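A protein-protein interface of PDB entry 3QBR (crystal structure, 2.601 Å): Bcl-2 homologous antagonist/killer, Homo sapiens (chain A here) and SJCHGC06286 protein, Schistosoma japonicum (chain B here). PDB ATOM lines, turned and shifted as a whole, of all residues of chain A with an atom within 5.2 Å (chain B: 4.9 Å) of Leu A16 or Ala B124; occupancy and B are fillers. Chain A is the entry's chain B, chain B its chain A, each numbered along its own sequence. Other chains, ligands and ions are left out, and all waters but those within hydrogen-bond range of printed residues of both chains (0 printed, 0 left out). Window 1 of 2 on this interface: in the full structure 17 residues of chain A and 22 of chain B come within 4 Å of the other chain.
The backbone NH of Leu B113 lies close to the backbone carbonyl oxygen of Gly A13 (3.5 Å).
The backbone carbonyl oxygen (O) of Leu B113 sits at hydrogen-bond distance from the guanidinium group (NH1) of Arg B121 (3.0 Å). The backbone NH (N) of Val A12 lies within hydrogen-bond range of the side-chain amide oxygen (OE1) of Gln A15, 3.1 Å away.
Among the printed residues, pairs that only touch across the chains: Gly A13 with Ile B109, Gly A20 with Gly B120, Ile A19 with Phe B72, Leu A16 with Ile B109, Ala A17 with Leu B113, Ala A17 with Arg B121, Ile A19 with Phe B76, Leu A16 with Phe B128, Val A12 with Ile B109, Leu A16 with Leu B113, Leu A16 with Phe B72 and Leu A16 with Ala B124.
Of the printed residues of chain B, Gly A13 touches Ile B109 and Leu B113. Leu A16 touches five residues of chain B. Ile A18 touches none of the printed residues of chain B. Printed residues of chain B within 4 Å of Gly A20: Gly B120 (3.2 Å). Of the printed residues of chain A, Leu B113 touches Gly A13 (3.0 Å), Leu A16 (3.9 Å) and Ala A17 (3.6 Å). Ala B124 touches just one residue of chain A: Leu A16. Of the printed residues of chain A, Phe B128 touches Leu A16 (3.8 Å). The nearest residue of chain B that does not touch Leu A16 is Phe B76 (4.6 Å). The nearest residue of chain A that does not touch Ala B124 is Gly A20 (4.5 Å). The nearest printed residue of chain A that does not touch Arg B121 is Gly A20 (4.02 Å).
Of the 9 printed residues of chain A, 6 touch a printed residue of chain B. Along chain A the printed residues that touch a printed residue of chain B span positions 12 to 20. Hydrophobic or aromatic side chains of chain B that line the printed part of chain A: Phe B72, Phe B76, Ile B109, Leu B113, Ala B124 and Phe B128. Among the printed residues, 13 pairs touch across the chains.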
ATOM      1  N   VAL A  12     -14.320  29.264   4.048  1.00  0.00           N
ATOM      2  CA  VAL A  12     -15.387  28.494   3.422  1.00  0.00           C
ATOM      3  C   VAL A  12     -14.930  27.717   2.174  1.00  0.00           C
ATOM      4  O   VAL A  12     -15.168  26.507   2.066  1.00  0.00           O
ATOM      5  CB  VAL A  12     -16.533  29.427   3.014  1.00  0.00           C
ATOM      6  CG1 VAL A  12     -17.809  28.643   2.840  1.00  0.00           C
ATOM      7  CG2 VAL A  12     -16.712  30.534   4.043  1.00  0.00           C
ATOM      8  N   GLY A  13     -14.277  28.417   1.244  1.00  0.00           N
ATOM      9  CA  GLY A  13     -13.791  27.802   0.019  1.00  0.00           C
ATOM     10  C   GLY A  13     -12.892  26.584   0.211  1.00  0.00           C
ATOM     11  O   GLY A  13     -12.863  25.662  -0.624  1.00  0.00           O
ATOM     12  N   ARG A  14     -12.140  26.569   1.309  1.00  0.00           N
ATOM     13  CA  ARG A  14     -11.223  25.459   1.547  1.00  0.00           C
ATOM     14  C   ARG A  14     -11.916  24.291   2.250  1.00  0.00           C
ATOM     15  O   ARG A  14     -11.528  23.128   2.051  1.00  0.00           O
ATOM     16  CB  ARG A  14      -9.996  25.938   2.303  1.00  0.00           C
ATOM     17  CG  ARG A  14      -9.615  27.367   1.955  1.00  0.00           C
ATOM     18  CD  ARG A  14      -8.409  27.859   2.769  1.00  0.00           C
ATOM     19  NE  ARG A  14      -8.276  29.317   2.733  1.00  0.00           N
ATOM     20  CZ  ARG A  14      -7.440  30.018   3.493  1.00  0.00           C
ATOM     21  NH1 ARG A  14      -6.648  29.402   4.362  1.00  0.00           N
ATOM     22  NH2 ARG A  14      -7.402  31.341   3.386  1.00  0.00           N
ATOM     23  N   GLN A  15     -12.947  24.590   3.054  1.00  0.00           N
ATOM     24  CA  GLN A  15     -13.814  23.529   3.588  1.00  0.00           C
ATOM     25  C   GLN A  15     -14.456  22.781   2.428  1.00  0.00           C
ATOM     26  O   GLN A  15     -14.498  21.549   2.406  1.00  0.00           O
ATOM     27  CB  GLN A  15     -14.915  24.076   4.497  1.00  0.00           C
ATOM     28  CG  GLN A  15     -14.541  24.212   5.968  1.00  0.00           C
ATOM     29  CD  GLN A  15     -14.253  25.656   6.371  1.00  0.00           C
ATOM     30  OE1 GLN A  15     -14.169  26.551   5.522  1.00  0.00           O
ATOM     31  NE2 GLN A  15     -14.105  25.886   7.676  1.00  0.00           N
ATOM     32  N   LEU A  16     -14.959  23.553   1.467  1.00  0.00           N
ATOM     33  CA  LEU A  16     -15.497  23.020   0.229  1.00  0.00           C
ATOM     34  C   LEU A  16     -14.387  22.281  -0.509  1.00  0.00           C
ATOM     35  O   LEU A  16     -14.604  21.199  -1.058  1.00  0.00           O
ATOM     36  CB  LEU A  16     -16.053  24.162  -0.628  1.00  0.00           C
ATOM     37  CG  LEU A  16     -17.238  24.970  -0.083  1.00  0.00           C
ATOM     38  CD1 LEU A  16     -17.435  26.249  -0.862  1.00  0.00           C
ATOM     39  CD2 LEU A  16     -18.510  24.146  -0.078  1.00  0.00           C
ATOM     40  N   ALA A  17     -13.188  22.856  -0.494  1.00  0.00           N
ATOM     41  CA  ALA A  17     -12.050  22.239  -1.174  1.00  0.00           C
ATOM     42  C   ALA A  17     -11.692  20.864  -0.645  1.00  0.00           C
ATOM     43  O   ALA A  17     -11.268  20.014  -1.420  1.00  0.00           O
ATOM     44  CB  ALA A  17     -10.845  23.135  -1.159  1.00  0.00           C
ATOM     45  N   ILE A  18     -11.854  20.611   0.649  1.00  0.00           N
ATOM     46  CA  ILE A  18     -11.449  19.279   1.116  1.00  0.00           C
ATOM     47  C   ILE A  18     -12.358  18.199   0.554  1.00  0.00           C
ATOM     48  O   ILE A  18     -11.878  17.168   0.072  1.00  0.00           O
ATOM     49  CB  ILE A  18     -11.250  19.115   2.672  1.00  0.00           C
ATOM     50  CG1 ILE A  18     -12.575  18.878   3.382  1.00  0.00           C
ATOM     51  CG2 ILE A  18     -10.469  20.283   3.284  1.00  0.00           C
ATOM     52  CD1 ILE A  18     -12.414  18.299   4.766  1.00  0.00           C
ATOM     53  N   ILE A  19     -13.666  18.445   0.598  1.00  0.00           N
ATOM     54  CA  ILE A  19     -14.630  17.520   0.000  1.00  0.00           C
ATOM     55  C   ILE A  19     -14.286  17.292  -1.468  1.00  0.00           C
ATOM     56  O   ILE A  19     -14.356  16.163  -1.964  1.00  0.00           O
ATOM     57  CB  ILE A  19     -16.083  18.046   0.113  1.00  0.00           C
ATOM     58  CG1 ILE A  19     -16.459  18.247   1.579  1.00  0.00           C
ATOM     59  CG2 ILE A  19     -17.056  17.087  -0.559  1.00  0.00           C
ATOM     60  CD1 ILE A  19     -17.897  18.658   1.800  1.00  0.00           C
ATOM     61  N   GLY A  20     -13.901  18.377  -2.149  1.00  0.00           N
ATOM     62  CA  GLY A  20     -13.499  18.321  -3.547  1.00  0.00           C
ATOM     63  C   GLY A  20     -12.330  17.383  -3.776  1.00  0.00           C
ATOM     64  O   GLY A  20     -12.333  16.552  -4.694  1.00  0.00           O
ATOM     65  N   PHE B  72     -20.859  14.547  -3.512  1.00  0.00           N
ATOM     66  CA  PHE B  72     -20.575  15.711  -2.681  1.00  0.00           C
ATOM     67  C   PHE B  72     -21.618  15.915  -1.590  1.00  0.00           C
ATOM     68  O   PHE B  72     -21.269  16.171  -0.446  1.00  0.00           O
ATOM     69  CB  PHE B  72     -20.440  16.981  -3.538  1.00  0.00           C
ATOM     70  CG  PHE B  72     -20.226  18.236  -2.747  1.00  0.00           C
ATOM     71  CD1 PHE B  72     -18.990  18.851  -2.730  1.00  0.00           C
ATOM     72  CD2 PHE B  72     -21.263  18.817  -2.050  1.00  0.00           C
ATOM     73  CE1 PHE B  72     -18.775  20.020  -2.013  1.00  0.00           C
ATOM     74  CE2 PHE B  72     -21.063  20.006  -1.323  1.00  0.00           C
ATOM     75  CZ  PHE B  72     -19.819  20.606  -1.312  1.00  0.00           C
ATOM     76  N   PHE B  76     -21.264  16.093   2.572  1.00  0.00           N
ATOM     77  CA  PHE B  76     -21.302  17.421   3.174  1.00  0.00           C
ATOM     78  C   PHE B  76     -22.377  17.517   4.251  1.00  0.00           C
ATOM     79  O   PHE B  76     -22.289  18.338   5.167  1.00  0.00           O
ATOM     80  CB  PHE B  76     -21.520  18.463   2.076  1.00  0.00           C
ATOM     81  CG  PHE B  76     -21.959  19.817   2.571  1.00  0.00           C
ATOM     82  CD1 PHE B  76     -21.135  20.925   2.417  1.00  0.00           C
ATOM     83  CD2 PHE B  76     -23.202  19.994   3.156  1.00  0.00           C
ATOM     84  CE1 PHE B  76     -21.538  22.184   2.850  1.00  0.00           C
ATOM     85  CE2 PHE B  76     -23.609  21.248   3.597  1.00  0.00           C
ATOM     86  CZ  PHE B  76     -22.782  22.340   3.436  1.00  0.00           C
ATOM     87  N   ILE B 109     -15.019  33.006  -1.818  1.00  0.00           N
ATOM     88  CA  ILE B 109     -15.193  31.574  -1.600  1.00  0.00           C
ATOM     89  C   ILE B 109     -14.639  30.744  -2.764  1.00  0.00           C
ATOM     90  O   ILE B 109     -14.052  29.681  -2.557  1.00  0.00           O
ATOM     91  CB  ILE B 109     -16.663  31.210  -1.418  1.00  0.00           C
ATOM     92  CG1 ILE B 109     -17.254  31.971  -0.236  1.00  0.00           C
ATOM     93  CG2 ILE B 109     -16.815  29.702  -1.242  1.00  0.00           C
ATOM     94  CD1 ILE B 109     -18.556  31.407   0.241  1.00  0.00           C
ATOM     95  N   LEU B 113     -11.792  28.184  -2.780  1.00  0.00           N
ATOM     96  CA  LEU B 113     -12.007  26.835  -3.302  1.00  0.00           C
ATOM     97  C   LEU B 113     -10.937  26.440  -4.317  1.00  0.00           C
ATOM     98  O   LEU B 113     -10.572  25.264  -4.441  1.00  0.00           O
ATOM     99  CB  LEU B 113     -13.399  26.714  -3.952  1.00  0.00           C
ATOM    100  CG  LEU B 113     -13.692  25.396  -4.695  1.00  0.00           C
ATOM    101  CD1 LEU B 113     -13.552  24.151  -3.809  1.00  0.00           C
ATOM    102  CD2 LEU B 113     -15.068  25.419  -5.343  1.00  0.00           C
ATOM    103  N   GLY B 120     -12.564  17.426  -8.894  1.00  0.00           N
ATOM    104  CA  GLY B 120     -13.297  17.381  -7.642  1.00  0.00           C
ATOM    105  C   GLY B 120     -13.673  18.751  -7.085  1.00  0.00           C
ATOM    106  O   GLY B 120     -14.744  18.933  -6.509  1.00  0.00           O
ATOM    107  N   ARG B 121     -12.780  19.716  -7.243  1.00  0.00           N
ATOM    108  CA  ARG B 121     -13.018  21.063  -6.762  1.00  0.00           C
ATOM    109  C   ARG B 121     -14.021  21.796  -7.652  1.00  0.00           C
ATOM    110  O   ARG B 121     -14.747  22.691  -7.184  1.00  0.00           O
ATOM    111  CB  ARG B 121     -11.699  21.853  -6.711  1.00  0.00           C
ATOM    112  CG  ARG B 121     -10.854  21.574  -5.480  1.00  0.00           C
ATOM    113  CD  ARG B 121      -9.374  21.995  -5.669  1.00  0.00           C
ATOM    114  NE  ARG B 121      -8.578  21.502  -4.553  1.00  0.00           N
ATOM    115  CZ  ARG B 121      -8.064  22.262  -3.593  1.00  0.00           C
ATOM    116  NH1 ARG B 121      -8.207  23.583  -3.621  1.00  0.00           N
ATOM    117  NH2 ARG B 121      -7.395  21.685  -2.602  1.00  0.00           N
ATOM    118  N   ILE B 122     -14.047  21.434  -8.935  1.00  0.00           N
ATOM    119  CA  ILE B 122     -15.001  22.045  -9.852  1.00  0.00           C
ATOM    120  C   ILE B 122     -16.423  21.570  -9.494  1.00  0.00           C
ATOM    121  O   ILE B 122     -17.334  22.382  -9.283  1.00  0.00           O
ATOM    122  CB  ILE B 122     -14.586  21.805 -11.329  1.00  0.00           C
ATOM    123  CG1 ILE B 122     -13.419  22.732 -11.683  1.00  0.00           C
ATOM    124  CG2 ILE B 122     -15.738  22.043 -12.276  1.00  0.00           C
ATOM    125  CD1 ILE B 122     -12.613  22.295 -12.910  1.00  0.00           C
ATOM    126  N   VAL B 123     -16.580  20.256  -9.378  1.00  0.00           N
ATOM    127  CA  VAL B 123     -17.783  19.645  -8.824  1.00  0.00           C
ATOM    128  C   VAL B 123     -18.293  20.380  -7.598  1.00  0.00           C
ATOM    129  O   VAL B 123     -19.480  20.708  -7.484  1.00  0.00           O
ATOM    130  CB  VAL B 123     -17.517  18.197  -8.402  1.00  0.00           C
ATOM    131  CG1 VAL B 123     -18.591  17.746  -7.458  1.00  0.00           C
ATOM    132  CG2 VAL B 123     -17.442  17.288  -9.616  1.00  0.00           C
ATOM    133  N   ALA B 124     -17.385  20.634  -6.670  1.00  0.00           N
ATOM    134  CA  ALA B 124     -17.749  21.337  -5.455  1.00  0.00           C
ATOM    135  C   ALA B 124     -18.339  22.717  -5.756  1.00  0.00           C
ATOM    136  O   ALA B 124     -19.183  23.198  -5.024  1.00  0.00           O
ATOM    137  CB  ALA B 124     -16.538  21.442  -4.528  1.00  0.00           C
ATOM    138  N   MET B 125     -17.895  23.361  -6.826  1.00  0.00           N
ATOM    139  CA  MET B 125     -18.458  24.661  -7.223  1.00  0.00           C
ATOM    140  C   MET B 125     -19.925  24.546  -7.698  1.00  0.00           C
ATOM    141  O   MET B 125     -20.762  25.382  -7.359  1.00  0.00           O
ATOM    142  CB  MET B 125     -17.595  25.297  -8.316  1.00  0.00           C
ATOM    143  CG  MET B 125     -18.145  26.582  -8.900  1.00  0.00           C
ATOM    144  SD  MET B 125     -17.226  27.213 -10.324  1.00  0.00           S
ATOM    145  CE  MET B 125     -17.147  25.767 -11.361  1.00  0.00           C
ATOM    146  N   PHE B 126     -20.237  23.508  -8.474  1.00  0.00           N
ATOM    147  CA  PHE B 126     -21.621  23.274  -8.860  1.00  0.00           C
ATOM    148  C   PHE B 126     -22.500  22.866  -7.684  1.00  0.00           C
ATOM    149  O   PHE B 126     -23.656  23.290  -7.603  1.00  0.00           O
ATOM    150  CB  PHE B 126     -21.739  22.215  -9.962  1.00  0.00           C
ATOM    151  CG  PHE B 126     -21.216  22.668 -11.307  1.00  0.00           C
ATOM    152  CD1 PHE B 126     -22.068  23.261 -12.239  1.00  0.00           C
ATOM    153  CD2 PHE B 126     -19.873  22.498 -11.646  1.00  0.00           C
ATOM    154  CE1 PHE B 126     -21.593  23.686 -13.504  1.00  0.00           C
ATOM    155  CE2 PHE B 126     -19.388  22.917 -12.898  1.00  0.00           C
ATOM    156  CZ  PHE B 126     -20.255  23.513 -13.837  1.00  0.00           C
ATOM    157  N   ALA B 127     -21.980  22.031  -6.786  1.00  0.00           N
ATOM    158  CA  ALA B 127     -22.827  21.533  -5.705  1.00  0.00           C
ATOM    159  C   ALA B 127     -23.178  22.679  -4.758  1.00  0.00           C
ATOM    160  O   ALA B 127     -24.322  22.789  -4.262  1.00  0.00           O
ATOM    161  CB  ALA B 127     -22.169  20.392  -4.972  1.00  0.00           C
ATOM    162  N   PHE B 128     -22.199  23.560  -4.560  1.00  0.00           N
ATOM    163  CA  PHE B 128     -22.379  24.715  -3.701  1.00  0.00           C
ATOM    164  C   PHE B 128     -23.275  25.773  -4.311  1.00  0.00           C
ATOM    165  O   PHE B 128     -24.142  26.325  -3.631  1.00  0.00           O
ATOM    166  CB  PHE B 128     -21.036  25.355  -3.392  1.00  0.00           C
ATOM    167  CG  PHE B 128     -21.097  26.439  -2.349  1.00  0.00           C
ATOM    168  CD1 PHE B 128     -21.551  26.169  -1.071  1.00  0.00           C
ATOM    169  CD2 PHE B 128     -20.637  27.708  -2.631  1.00  0.00           C
ATOM    170  CE1 PHE B 128     -21.574  27.173  -0.099  1.00  0.00           C
ATOM    171  CE2 PHE B 128     -20.642  28.711  -1.660  1.00  0.00           C
ATOM    172  CZ  PHE B 128     -21.118  28.441  -0.401  1.00  0.00           C
ATOM    173  N   LEU B 129     -23.028  26.098  -5.575  1.00  0.00           N
ATOM    174  CA  LEU B 129     -23.888  27.036  -6.315  1.00  0.00           C
ATOM    175  C   LEU B 129     -25.359  26.578  -6.266  1.00  0.00           C
ATOM    176  O   LEU B 129     -26.259  27.379  -6.030  1.00  0.00           O
ATOM    177  CB  LEU B 129     -23.402  27.166  -7.756  1.00  0.00           C
ATOM    178  CG  LEU B 129     -24.230  27.941  -8.781  1.00  0.00           C
ATOM    179  CD1 LEU B 129     -24.202  29.474  -8.556  1.00  0.00           C
ATOM    180  CD2 LEU B 129     -23.719  27.568 -10.181  1.00  0.00           C
